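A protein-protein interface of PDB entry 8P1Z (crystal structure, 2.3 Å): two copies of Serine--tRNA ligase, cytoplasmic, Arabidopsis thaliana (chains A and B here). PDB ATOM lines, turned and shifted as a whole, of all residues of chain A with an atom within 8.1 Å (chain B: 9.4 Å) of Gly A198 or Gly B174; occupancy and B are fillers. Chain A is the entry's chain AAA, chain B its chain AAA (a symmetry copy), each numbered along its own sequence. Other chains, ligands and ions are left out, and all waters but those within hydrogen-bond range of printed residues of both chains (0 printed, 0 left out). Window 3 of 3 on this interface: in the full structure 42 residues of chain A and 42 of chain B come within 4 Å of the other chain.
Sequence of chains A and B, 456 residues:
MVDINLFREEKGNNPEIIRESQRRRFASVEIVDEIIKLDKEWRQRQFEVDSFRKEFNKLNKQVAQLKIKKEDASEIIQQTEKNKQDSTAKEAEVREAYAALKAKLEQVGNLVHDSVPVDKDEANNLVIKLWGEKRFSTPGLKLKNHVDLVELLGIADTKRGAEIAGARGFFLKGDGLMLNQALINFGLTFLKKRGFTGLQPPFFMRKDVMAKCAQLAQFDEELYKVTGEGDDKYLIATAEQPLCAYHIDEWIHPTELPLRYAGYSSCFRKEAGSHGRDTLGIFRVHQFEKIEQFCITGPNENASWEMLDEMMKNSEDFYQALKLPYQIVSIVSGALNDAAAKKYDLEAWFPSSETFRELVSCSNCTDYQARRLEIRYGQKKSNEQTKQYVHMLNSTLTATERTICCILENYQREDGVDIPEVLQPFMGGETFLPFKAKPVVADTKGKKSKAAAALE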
ATOM      1  N   LEU A 188       3.372  16.724   1.398  1.00  0.00           N
ATOM      2  CA  LEU A 188       3.065  17.574   2.581  1.00  0.00           C
ATOM      3  C   LEU A 188       3.504  16.832   3.847  1.00  0.00           C
ATOM      4  O   LEU A 188       4.135  17.486   4.717  1.00  0.00           O
ATOM      5  CB  LEU A 188       1.572  17.955   2.618  1.00  0.00           C
ATOM      6  CG  LEU A 188       1.093  18.895   1.504  1.00  0.00           C
ATOM      7  CD1 LEU A 188      -0.389  19.165   1.587  1.00  0.00           C
ATOM      8  CD2 LEU A 188       1.834  20.222   1.508  1.00  0.00           C
ATOM      9  N   LEU A 191       7.399  16.592   4.092  1.00  0.00           N
ATOM     10  CA  LEU A 191       7.992  17.890   4.484  1.00  0.00           C
ATOM     11  C   LEU A 191       7.620  18.241   5.924  1.00  0.00           C
ATOM     12  O   LEU A 191       8.486  18.802   6.639  1.00  0.00           O
ATOM     13  CB  LEU A 191       7.538  18.973   3.498  1.00  0.00           C
ATOM     14  CG  LEU A 191       8.346  19.012   2.197  1.00  0.00           C
ATOM     15  CD1 LEU A 191       7.925  20.185   1.326  1.00  0.00           C
ATOM     16  CD2 LEU A 191       9.850  19.079   2.475  1.00  0.00           C
ATOM     17  N   LYS A 192       6.397  17.921   6.350  1.00  0.00           N
ATOM     18  CA  LYS A 192       5.948  18.192   7.741  1.00  0.00           C
ATOM     19  C   LYS A 192       6.863  17.415   8.688  1.00  0.00           C
ATOM     20  O   LYS A 192       7.205  17.968   9.750  1.00  0.00           O
ATOM     21  CB  LYS A 192       4.471  17.840   7.943  1.00  0.00           C
ATOM     22  CG  LYS A 192       3.912  18.224   9.306  1.00  0.00           C
ATOM     23  CD  LYS A 192       2.404  18.135   9.408  1.00  0.00           C
ATOM     24  CE  LYS A 192       1.899  18.483  10.793  1.00  0.00           C
ATOM     25  NZ  LYS A 192       2.000  17.327  11.716  1.00  0.00           N
ATOM     26  N   GLY A 195      10.142  19.485   9.537  1.00  0.00           N
ATOM     27  CA  GLY A 195      10.110  20.770  10.253  1.00  0.00           C
ATOM     28  C   GLY A 195       9.358  21.842   9.497  1.00  0.00           C
ATOM     29  O   GLY A 195       9.438  23.005   9.920  1.00  0.00           O
ATOM     30  N   PHE A 196       8.630  21.470   8.442  1.00  0.00           N
ATOM     31  CA  PHE A 196       7.871  22.419   7.587  1.00  0.00           C
ATOM     32  C   PHE A 196       6.434  22.565   8.099  1.00  0.00           C
ATOM     33  O   PHE A 196       5.836  21.591   8.644  1.00  0.00           O
ATOM     34  CB  PHE A 196       7.856  21.969   6.121  1.00  0.00           C
ATOM     35  CG  PHE A 196       9.129  22.235   5.357  1.00  0.00           C
ATOM     36  CD1 PHE A 196      10.292  21.531   5.646  1.00  0.00           C
ATOM     37  CD2 PHE A 196       9.159  23.176   4.336  1.00  0.00           C
ATOM     38  CE1 PHE A 196      11.463  21.779   4.944  1.00  0.00           C
ATOM     39  CE2 PHE A 196      10.328  23.421   3.629  1.00  0.00           C
ATOM     40  CZ  PHE A 196      11.477  22.720   3.932  1.00  0.00           C
ATOM     41  N   THR A 197       5.893  23.763   7.877  1.00  0.00           N
ATOM     42  CA  THR A 197       4.491  24.157   8.150  1.00  0.00           C
ATOM     43  C   THR A 197       3.806  24.349   6.806  1.00  0.00           C
ATOM     44  O   THR A 197       4.301  25.185   6.033  1.00  0.00           O
ATOM     45  CB  THR A 197       4.408  25.463   8.956  1.00  0.00           C
ATOM     46  OG1 THR A 197       4.842  25.221  10.291  1.00  0.00           O
ATOM     47  CG2 THR A 197       3.012  26.045   9.031  1.00  0.00           C
ATOM     48  N   GLY A 198       2.726  23.608   6.555  1.00  0.00           N
ATOM     49  CA  GLY A 198       1.865  23.758   5.370  1.00  0.00           C
ATOM     50  C   GLY A 198       1.385  25.189   5.227  1.00  0.00           C
ATOM     51  O   GLY A 198       1.174  25.844   6.250  1.00  0.00           O
ATOM     52  N   LEU A 199       1.267  25.661   3.987  1.00  0.00           N
ATOM     53  CA  LEU A 199       0.691  26.971   3.603  1.00  0.00           C
ATOM     54  C   LEU A 199       0.081  26.836   2.208  1.00  0.00           C
ATOM     55  O   LEU A 199       0.792  26.385   1.292  1.00  0.00           O
ATOM     56  CB  LEU A 199       1.781  28.041   3.601  1.00  0.00           C
ATOM     57  CG  LEU A 199       1.674  29.109   4.687  1.00  0.00           C
ATOM     58  CD1 LEU A 199       2.565  30.295   4.348  1.00  0.00           C
ATOM     59  CD2 LEU A 199       0.238  29.572   4.874  1.00  0.00           C
ATOM     60  N   GLN A 200      -1.195  27.190   2.059  1.00  0.00           N
ATOM     61  CA  GLN A 200      -1.876  27.224   0.744  1.00  0.00           C
ATOM     62  C   GLN A 200      -2.258  28.663   0.483  1.00  0.00           C
ATOM     63  O   GLN A 200      -3.115  29.202   1.161  1.00  0.00           O
ATOM     64  CB  GLN A 200      -3.104  26.314   0.695  1.00  0.00           C
ATOM     65  CG  GLN A 200      -3.890  26.403  -0.612  1.00  0.00           C
ATOM     66  CD  GLN A 200      -4.981  25.360  -0.684  1.00  0.00           C
ATOM     67  OE1 GLN A 200      -4.961  24.361   0.034  1.00  0.00           O
ATOM     68  NE2 GLN A 200      -5.946  25.581  -1.561  1.00  0.00           N
ATOM     69  N   PRO A 201      -1.628  29.332  -0.500  1.00  0.00           N
ATOM     70  CA  PRO A 201      -1.908  30.737  -0.730  1.00  0.00           C
ATOM     71  C   PRO A 201      -3.164  30.869  -1.570  1.00  0.00           C
ATOM     72  O   PRO A 201      -3.645  29.883  -2.140  1.00  0.00           O
ATOM     73  CB  PRO A 201      -0.690  31.190  -1.525  1.00  0.00           C
ATOM     74  CG  PRO A 201      -0.338  29.978  -2.338  1.00  0.00           C
ATOM     75  CD  PRO A 201      -0.639  28.796  -1.442  1.00  0.00           C
ATOM     76  N   LEU A 243       4.080  33.139  -1.444  1.00  0.00           N
ATOM     77  CA  LEU A 243       5.051  32.860  -0.347  1.00  0.00           C
ATOM     78  C   LEU A 243       6.336  33.648  -0.609  1.00  0.00           C
ATOM     79  O   LEU A 243       7.346  33.057  -0.999  1.00  0.00           O
ATOM     80  CB  LEU A 243       5.363  31.367  -0.283  1.00  0.00           C
ATOM     81  CG  LEU A 243       4.305  30.483   0.358  1.00  0.00           C
ATOM     82  CD1 LEU A 243       2.965  30.596  -0.366  1.00  0.00           C
ATOM     83  CD2 LEU A 243       4.802  29.043   0.388  1.00  0.00           C
ATOM     84  N   TYR A 246       3.972  37.213   1.506  1.00  0.00           N
ATOM     85  CA  TYR A 246       3.764  36.829   2.931  1.00  0.00           C
ATOM     86  C   TYR A 246       5.031  37.215   3.682  1.00  0.00           C
ATOM     87  O   TYR A 246       6.112  36.751   3.237  1.00  0.00           O
ATOM     88  CB  TYR A 246       3.529  35.323   3.071  1.00  0.00           C
ATOM     89  CG  TYR A 246       3.019  34.790   4.393  1.00  0.00           C
ATOM     90  CD1 TYR A 246       3.838  34.630   5.503  1.00  0.00           C
ATOM     91  CD2 TYR A 246       1.724  34.307   4.495  1.00  0.00           C
ATOM     92  CE1 TYR A 246       3.370  34.071   6.684  1.00  0.00           C
ATOM     93  CE2 TYR A 246       1.233  33.756   5.666  1.00  0.00           C
ATOM     94  CZ  TYR A 246       2.057  33.632   6.768  1.00  0.00           C
ATOM     95  OH  TYR A 246       1.527  33.090   7.910  1.00  0.00           O
ATOM     96  N   ARG A 260      10.411  27.308   7.792  1.00  0.00           N
ATOM     97  CA  ARG A 260      10.198  26.296   6.730  1.00  0.00           C
ATOM     98  C   ARG A 260       8.702  26.219   6.419  1.00  0.00           C
ATOM     99  O   ARG A 260       7.945  25.765   7.281  1.00  0.00           O
ATOM    100  CB  ARG A 260      10.757  24.942   7.170  1.00  0.00           C
ATOM    101  CG  ARG A 260      12.158  25.011   7.752  1.00  0.00           C
ATOM    102  CD  ARG A 260      12.650  23.612   8.068  1.00  0.00           C
ATOM    103  NE  ARG A 260      14.085  23.585   8.277  1.00  0.00           N
ATOM    104  CZ  ARG A 260      14.708  23.856   9.414  1.00  0.00           C
ATOM    105  NH1 ARG A 260      14.031  24.185  10.498  1.00  0.00           N
ATOM    106  NH2 ARG A 260      16.030  23.813   9.461  1.00  0.00           N
ATOM    107  N   TYR A 261       8.311  26.643   5.221  1.00  0.00           N
ATOM    108  CA  TYR A 261       6.943  26.520   4.675  1.00  0.00           C
ATOM    109  C   TYR A 261       6.915  25.520   3.514  1.00  0.00           C
ATOM    110  O   TYR A 261       7.702  25.674   2.533  1.00  0.00           O
ATOM    111  CB  TYR A 261       6.462  27.879   4.174  1.00  0.00           C
ATOM    112  CG  TYR A 261       6.456  28.971   5.207  1.00  0.00           C
ATOM    113  CD1 TYR A 261       5.916  28.765   6.464  1.00  0.00           C
ATOM    114  CD2 TYR A 261       6.927  30.237   4.905  1.00  0.00           C
ATOM    115  CE1 TYR A 261       5.878  29.775   7.410  1.00  0.00           C
ATOM    116  CE2 TYR A 261       6.899  31.258   5.839  1.00  0.00           C
ATOM    117  CZ  TYR A 261       6.371  31.029   7.098  1.00  0.00           C
ATOM    118  OH  TYR A 261       6.334  32.028   8.028  1.00  0.00           O
ATOM    119  N   ALA A 262       6.009  24.545   3.603  1.00  0.00           N
ATOM    120  CA  ALA A 262       5.604  23.668   2.485  1.00  0.00           C
ATOM    121  C   ALA A 262       4.457  24.334   1.729  1.00  0.00           C
ATOM    122  O   ALA A 262       3.274  24.097   2.095  1.00  0.00           O
ATOM    123  CB  ALA A 262       5.199  22.302   2.988  1.00  0.00           C
ATOM    124  N   GLY A 263       4.783  25.132   0.709  1.00  0.00           N
ATOM    125  CA  GLY A 263       3.781  25.841  -0.110  1.00  0.00           C
ATOM    126  C   GLY A 263       2.970  24.851  -0.920  1.00  0.00           C
ATOM    127  O   GLY A 263       3.588  24.006  -1.534  1.00  0.00           O
ATOM    128  N   TYR A 264       1.638  24.893  -0.898  1.00  0.00           N
ATOM    129  CA  TYR A 264       0.831  24.073  -1.842  1.00  0.00           C
ATOM    130  C   TYR A 264      -0.115  24.989  -2.625  1.00  0.00           C
ATOM    131  O   TYR A 264      -0.717  25.861  -2.006  1.00  0.00           O
ATOM    132  CB  TYR A 264       0.091  22.935  -1.136  1.00  0.00           C
ATOM    133  CG  TYR A 264      -0.992  22.381  -2.015  1.00  0.00           C
ATOM    134  CD1 TYR A 264      -0.674  21.694  -3.169  1.00  0.00           C
ATOM    135  CD2 TYR A 264      -2.334  22.631  -1.761  1.00  0.00           C
ATOM    136  CE1 TYR A 264      -1.660  21.230  -4.024  1.00  0.00           C
ATOM    137  CE2 TYR A 264      -3.331  22.160  -2.601  1.00  0.00           C
ATOM    138  CZ  TYR A 264      -2.989  21.460  -3.741  1.00  0.00           C
ATOM    139  OH  TYR A 264      -3.944  21.002  -4.596  1.00  0.00           O
ATOM    140  N   GLU A 292       6.090  23.315  -2.977  1.00  0.00           N
ATOM    141  CA  GLU A 292       7.317  24.142  -3.017  1.00  0.00           C
ATOM    142  C   GLU A 292       7.919  24.133  -1.621  1.00  0.00           C
ATOM    143  O   GLU A 292       7.151  24.227  -0.673  1.00  0.00           O
ATOM    144  CB  GLU A 292       7.005  25.579  -3.433  1.00  0.00           C
ATOM    145  CG  GLU A 292       7.035  25.790  -4.932  1.00  0.00           C
ATOM    146  CD  GLU A 292       8.433  25.852  -5.521  1.00  0.00           C
ATOM    147  OE1 GLU A 292       9.356  26.336  -4.822  1.00  0.00           O
ATOM    148  OE2 GLU A 292       8.604  25.419  -6.682  1.00  0.00           O
ATOM    149  N   LEU B 153      -7.040  29.063  16.538  1.00  0.00           N
ATOM    150  CA  LEU B 153      -6.399  27.787  16.112  1.00  0.00           C
ATOM    151  C   LEU B 153      -5.121  28.065  15.310  1.00  0.00           C
ATOM    152  O   LEU B 153      -4.251  27.179  15.291  1.00  0.00           O
ATOM    153  CB  LEU B 153      -7.400  26.952  15.305  1.00  0.00           C
ATOM    154  CG  LEU B 153      -8.498  26.300  16.145  1.00  0.00           C
ATOM    155  CD1 LEU B 153      -9.596  25.724  15.265  1.00  0.00           C
ATOM    156  CD2 LEU B 153      -7.924  25.230  17.060  1.00  0.00           C
ATOM    157  N   GLY B 154      -5.014  29.248  14.703  1.00  0.00           N
ATOM    158  CA  GLY B 154      -3.900  29.645  13.824  1.00  0.00           C
ATOM    159  C   GLY B 154      -3.842  28.815  12.553  1.00  0.00           C
ATOM    160  O   GLY B 154      -2.729  28.370  12.197  1.00  0.00           O
ATOM    161  N   ILE B 155      -4.965  28.622  11.856  1.00  0.00           N
ATOM    162  CA  ILE B 155      -5.018  27.700  10.680  1.00  0.00           C
ATOM    163  C   ILE B 155      -5.350  28.441   9.377  1.00  0.00           C
ATOM    164  O   ILE B 155      -5.427  27.784   8.337  1.00  0.00           O
ATOM    165  CB  ILE B 155      -5.992  26.555  10.957  1.00  0.00           C
ATOM    166  CG1 ILE B 155      -7.417  27.048  11.187  1.00  0.00           C
ATOM    167  CG2 ILE B 155      -5.475  25.732  12.123  1.00  0.00           C
ATOM    168  CD1 ILE B 155      -8.416  25.929  11.328  1.00  0.00           C
ATOM    169  N   ALA B 156      -5.528  29.756   9.415  1.00  0.00           N
ATOM    170  CA  ALA B 156      -5.708  30.568   8.199  1.00  0.00           C
ATOM    171  C   ALA B 156      -5.153  31.955   8.464  1.00  0.00           C
ATOM    172  O   ALA B 156      -5.478  32.505   9.528  1.00  0.00           O
ATOM    173  CB  ALA B 156      -7.161  30.644   7.810  1.00  0.00           C
ATOM    174  N   ASP B 157      -4.359  32.485   7.541  1.00  0.00           N
ATOM    175  CA  ASP B 157      -3.962  33.908   7.581  1.00  0.00           C
ATOM    176  C   ASP B 157      -4.884  34.655   6.631  1.00  0.00           C
ATOM    177  O   ASP B 157      -4.596  34.676   5.421  1.00  0.00           O
ATOM    178  CB  ASP B 157      -2.483  34.127   7.270  1.00  0.00           C
ATOM    179  CG  ASP B 157      -1.952  35.371   7.959  1.00  0.00           C
ATOM    180  OD1 ASP B 157      -2.644  36.424   7.876  1.00  0.00           O
ATOM    181  OD2 ASP B 157      -0.869  35.270   8.596  1.00  0.00           O
ATOM    182  N   PHE B 171      -4.838  32.515   3.253  1.00  0.00           N
ATOM    183  CA  PHE B 171      -3.981  31.302   3.264  1.00  0.00           C
ATOM    184  C   PHE B 171      -4.646  30.231   4.130  1.00  0.00           C
ATOM    185  O   PHE B 171      -5.201  30.599   5.152  1.00  0.00           O
ATOM    186  CB  PHE B 171      -2.603  31.628   3.833  1.00  0.00           C
ATOM    187  CG  PHE B 171      -1.747  32.525   2.977  1.00  0.00           C
ATOM    188  CD1 PHE B 171      -2.001  33.885   2.895  1.00  0.00           C
ATOM    189  CD2 PHE B 171      -0.674  32.011   2.264  1.00  0.00           C
ATOM    190  CE1 PHE B 171      -1.205  34.710   2.115  1.00  0.00           C
ATOM    191  CE2 PHE B 171       0.130  32.841   1.499  1.00  0.00           C
ATOM    192  CZ  PHE B 171      -0.140  34.186   1.421  1.00  0.00           C
ATOM    193  N   LEU B 172      -4.637  28.961   3.722  1.00  0.00           N
ATOM    194  CA  LEU B 172      -4.780  27.827   4.675  1.00  0.00           C
ATOM    195  C   LEU B 172      -3.389  27.550   5.244  1.00  0.00           C
ATOM    196  O   LEU B 172      -2.419  27.743   4.516  1.00  0.00           O
ATOM    197  CB  LEU B 172      -5.364  26.585   3.998  1.00  0.00           C
ATOM    198  CG  LEU B 172      -6.866  26.614   3.703  1.00  0.00           C
ATOM    199  CD1 LEU B 172      -7.321  25.313   3.039  1.00  0.00           C
ATOM    200  CD2 LEU B 172      -7.679  26.870   4.955  1.00  0.00           C
ATOM    201  N   LYS B 173      -3.301  27.150   6.507  1.00  0.00           N
ATOM    202  CA  LYS B 173      -2.010  27.039   7.230  1.00  0.00           C
ATOM    203  C   LYS B 173      -2.031  25.822   8.153  1.00  0.00           C
ATOM    204  O   LYS B 173      -3.111  25.440   8.610  1.00  0.00           O
ATOM    205  CB  LYS B 173      -1.725  28.318   8.015  1.00  0.00           C
ATOM    206  CG  LYS B 173      -0.350  28.378   8.661  1.00  0.00           C
ATOM    207  CD  LYS B 173       0.097  29.790   9.053  1.00  0.00           C
ATOM    208  CE  LYS B 173       1.390  29.781   9.850  1.00  0.00           C
ATOM    209  NZ  LYS B 173       2.195  31.006   9.636  1.00  0.00           N
ATOM    210  N   GLY B 174      -0.856  25.233   8.373  1.00  0.00           N
ATOM    211  CA  GLY B 174      -0.644  24.111   9.301  1.00  0.00           C
ATOM    212  C   GLY B 174      -1.782  23.127   9.222  1.00  0.00           C
ATOM    213  O   GLY B 174      -2.099  22.666   8.109  1.00  0.00           O
ATOM    214  N   ASP B 175      -2.425  22.856  10.348  1.00  0.00           N
ATOM    215  CA  ASP B 175      -3.486  21.825  10.421  1.00  0.00           C
ATOM    216  C   ASP B 175      -4.732  22.286   9.647  1.00  0.00           C
ATOM    217  O   ASP B 175      -5.592  21.412   9.389  1.00  0.00           O
ATOM    218  CB  ASP B 175      -3.753  21.439  11.873  1.00  0.00           C
ATOM    219  CG  ASP B 175      -2.615  20.633  12.480  1.00  0.00           C
ATOM    220  OD1 ASP B 175      -2.285  19.558  11.920  1.00  0.00           O
ATOM    221  OD2 ASP B 175      -2.054  21.092  13.496  1.00  0.00           O
ATOM    222  N   GLY B 176      -4.831  23.563   9.255  1.00  0.00           N
ATOM    223  CA  GLY B 176      -5.902  24.056   8.364  1.00  0.00           C
ATOM    224  C   GLY B 176      -5.850  23.390   6.991  1.00  0.00           C
ATOM    225  O   GLY B 176      -6.907  22.942   6.476  1.00  0.00           O
ATOM    226  N   LEU B 177      -4.649  23.314   6.414  1.00  0.00           N
ATOM    227  CA  LEU B 177      -4.396  22.694   5.089  1.00  0.00           C
ATOM    228  C   LEU B 177      -4.631  21.185   5.214  1.00  0.00           C
ATOM    229  O   LEU B 177      -5.404  20.644   4.387  1.00  0.00           O
ATOM    230  CB  LEU B 177      -2.968  23.037   4.641  1.00  0.00           C
ATOM    231  CG  LEU B 177      -2.540  22.500   3.274  1.00  0.00           C
ATOM    232  CD1 LEU B 177      -3.640  22.676   2.238  1.00  0.00           C
ATOM    233  CD2 LEU B 177      -1.264  23.184   2.807  1.00  0.00           C
ATOM    234  N   MET B 178      -4.028  20.546   6.226  1.00  0.00           N
ATOM    235  CA  MET B 178      -4.195  19.093   6.520  1.00  0.00           C
ATOM    236  C   MET B 178      -5.691  18.762   6.606  1.00  0.00           C
ATOM    237  O   MET B 178      -6.097  17.710   6.080  1.00  0.00           O
ATOM    238  CB  MET B 178      -3.514  18.710   7.840  1.00  0.00           C
ATOM    239  CG  MET B 178      -3.162  17.230   7.952  1.00  0.00           C
ATOM    240  SD  MET B 178      -2.247  16.802   9.472  1.00  0.00           S
ATOM    241  CE  MET B 178      -1.407  15.318   8.920  1.00  0.00           C
ATOM    242  N   LEU B 179      -6.477  19.634   7.263  1.00  0.00           N
ATOM    243  CA  LEU B 179      -7.946  19.428   7.446  1.00  0.00           C
ATOM    244  C   LEU B 179      -8.668  19.557   6.111  1.00  0.00           C
ATOM    245  O   LEU B 179      -9.492  18.682   5.785  1.00  0.00           O
ATOM    246  CB  LEU B 179      -8.539  20.446   8.423  1.00  0.00           C
ATOM    247  CG  LEU B 179      -9.128  19.873   9.709  1.00  0.00           C
ATOM    248  CD1 LEU B 179     -10.013  20.908  10.379  1.00  0.00           C
ATOM    249  CD2 LEU B 179      -9.908  18.596   9.454  1.00  0.00           C
ATOM    250  N   ASN B 180      -8.399  20.651   5.406  1.00  0.00           N
ATOM    251  CA  ASN B 180      -8.964  20.883   4.061  1.00  0.00           C
ATOM    252  C   ASN B 180      -8.714  19.622   3.229  1.00  0.00           C
ATOM    253  O   ASN B 180      -9.670  19.126   2.576  1.00  0.00           O
ATOM    254  CB  ASN B 180      -8.368  22.143   3.433  1.00  0.00           C
ATOM    255  CG  ASN B 180      -9.189  22.638   2.267  1.00  0.00           C
ATOM    256  OD1 ASN B 180     -10.381  22.889   2.406  1.00  0.00           O
ATOM    257  ND2 ASN B 180      -8.556  22.787   1.124  1.00  0.00           N
ATOM    258  N   GLN B 181      -7.477  19.118   3.272  1.00  0.00           N
ATOM    259  CA  GLN B 181      -7.029  17.965   2.448  1.00  0.00           C
ATOM    260  C   GLN B 181      -7.700  16.689   2.969  1.00  0.00           C
ATOM    261  O   GLN B 181      -8.118  15.856   2.131  1.00  0.00           O
ATOM    262  CB  GLN B 181      -5.500  17.857   2.452  1.00  0.00           C
ATOM    263  CG  GLN B 181      -4.782  18.813   1.492  1.00  0.00           C
ATOM    264  CD  GLN B 181      -5.234  18.658   0.058  1.00  0.00           C
ATOM    265  OE1 GLN B 181      -5.131  17.575  -0.531  1.00  0.00           O
ATOM    266  NE2 GLN B 181      -5.738  19.746  -0.521  1.00  0.00           N
ATOM    267  N   ALA B 182      -7.836  16.562   4.293  1.00  0.00           N
ATOM    268  CA  ALA B 182      -8.509  15.434   4.974  1.00  0.00           C
ATOM    269  C   ALA B 182      -9.947  15.297   4.483  1.00  0.00           C
ATOM    270  O   ALA B 182     -10.402  14.174   4.218  1.00  0.00           O
ATOM    271  CB  ALA B 182      -8.486  15.664   6.453  1.00  0.00           C
ATOM    272  N   MET B 427      -5.624  12.719   8.924  1.00  0.00           N
ATOM    273  CA  MET B 427      -4.859  13.763   9.662  1.00  0.00           C
ATOM    274  C   MET B 427      -3.775  13.088  10.498  1.00  0.00           C
ATOM    275  O   MET B 427      -3.290  13.736  11.464  1.00  0.00           O
ATOM    276  CB  MET B 427      -5.758  14.539  10.627  1.00  0.00           C
ATOM    277  CG  MET B 427      -6.881  15.318   9.973  1.00  0.00           C
ATOM    278  SD  MET B 427      -6.441  17.022   9.592  1.00  0.00           S
ATOM    279  CE  MET B 427      -5.693  17.599  11.113  1.00  0.00           C
ATOM    280  N   GLU B 430      -4.388  12.296  14.685  1.00  0.00           N
ATOM    281  CA  GLU B 430      -4.528  13.470  15.600  1.00  0.00           C
ATOM    282  C   GLU B 430      -6.022  13.729  15.914  1.00  0.00           C
ATOM    283  O   GLU B 430      -6.857  13.712  14.991  1.00  0.00           O
ATOM    284  CB  GLU B 430      -3.811  14.677  14.971  1.00  0.00           C
ATOM    285  CG  GLU B 430      -3.329  15.722  15.973  1.00  0.00           C
ATOM    286  CD  GLU B 430      -1.982  16.361  15.644  1.00  0.00           C
ATOM    287  OE1 GLU B 430      -1.956  17.582  15.355  1.00  0.00           O
ATOM    288  OE2 GLU B 430      -0.955  15.639  15.697  1.00  0.00           O
ATOM    289  N   LEU B 433      -7.015  19.989  18.036  1.00  0.00           N
ATOM    290  CA  LEU B 433      -6.297  21.180  17.527  1.00  0.00           C
ATOM    291  C   LEU B 433      -6.317  22.220  18.633  1.00  0.00           C
ATOM    292  O   LEU B 433      -7.345  22.828  18.879  1.00  0.00           O
ATOM    293  CB  LEU B 433      -6.980  21.674  16.250  1.00  0.00           C
ATOM    294  CG  LEU B 433      -7.001  20.669  15.094  1.00  0.00           C
ATOM    295  CD1 LEU B 433      -7.981  21.095  14.013  1.00  0.00           C
ATOM    296  CD2 LEU B 433      -5.610  20.486  14.508  1.00  0.00           C
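The side-chain carboxylate (OD2) of Asp B157 lies within hydrogen-bond range of the side-chain hydroxyl (OH) of Tyr A246 (3.3 Å). The backbone carbonyl oxygen (O) of Gly A198 lies within hydrogen-bond range of the backbone NH (N) of Gly B174 (3.0 Å). The backbone NH (N) of Gln A200 lies within hydrogen-bond range of the backbone carbonyl oxygen (O) of Leu B172 (2.8 Å). The side-chain hydroxyl (OH) of Tyr A246 sits at hydrogen-bond distance from the side-chain amino group (NZ) of Lys B173 (2.8 Å).
Leu A199 touches four residues of chain B. Printed residues of chain B within 4 Å of Pro A201: Phe B171. No residue of chain B comes within 4 Å of Ala A262. Of the printed residues of chain A, Asp B157 touches Tyr A246 (3.3 Å). Of the printed residues of chain A, Phe B171 touches Leu A199, Gln A200, Pro A201 and Tyr A246. Of the printed residues of chain A, Gly B174 touches Gly A198. The nearest printed residue of chain A that does not touch Gly B174 is Thr A197 (4.01 Å).
No position is printed for both chains.
Of the 20 printed residues of chain B, 7 touch a printed residue of chain A. Hydrophobic or aromatic side chains of chain B that line the printed part of chain A: Phe B171, Leu B172 and Leu B177.
Lys B173 touches Gly A198. Phe B171 touches Leu A199 (CB to CD2, 3.7 Å). CD2 of Leu A199 touches O of Leu B172, at 3.2 Å. Leu A199 touches Lys B173. Leu B177 touches Leu A199. O of Gln A200 touches CA of Phe B171 (3.1 Å). OE1 of Gln A200 touches CD1 of Leu B177 (3.1 Å). Phe B171 touches Pro A201 (CD2 to CA, 3.5 Å). Phe B171 touches Tyr A246 (CZ to CD2, 3.6 Å). NE2 of Gln B181 touches CE2 of Tyr A264, 3.99 Å away.
The backbone carbonyl oxygen of Asp B157 lies within hydrogen-bond range of the backbone NH of Phe B171. N of Leu A199 lies within hydrogen-bond range of O of Ala A262. The backbone carbonyl oxygen (O) of Leu A199 is in hydrogen-bond range of the backbone NH (N) of Tyr A264. The backbone carbonyl oxygen (O) of Ile B155 is in hydrogen-bond range of the backbone NH (N) of Lys B173, at 2.9 Å.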
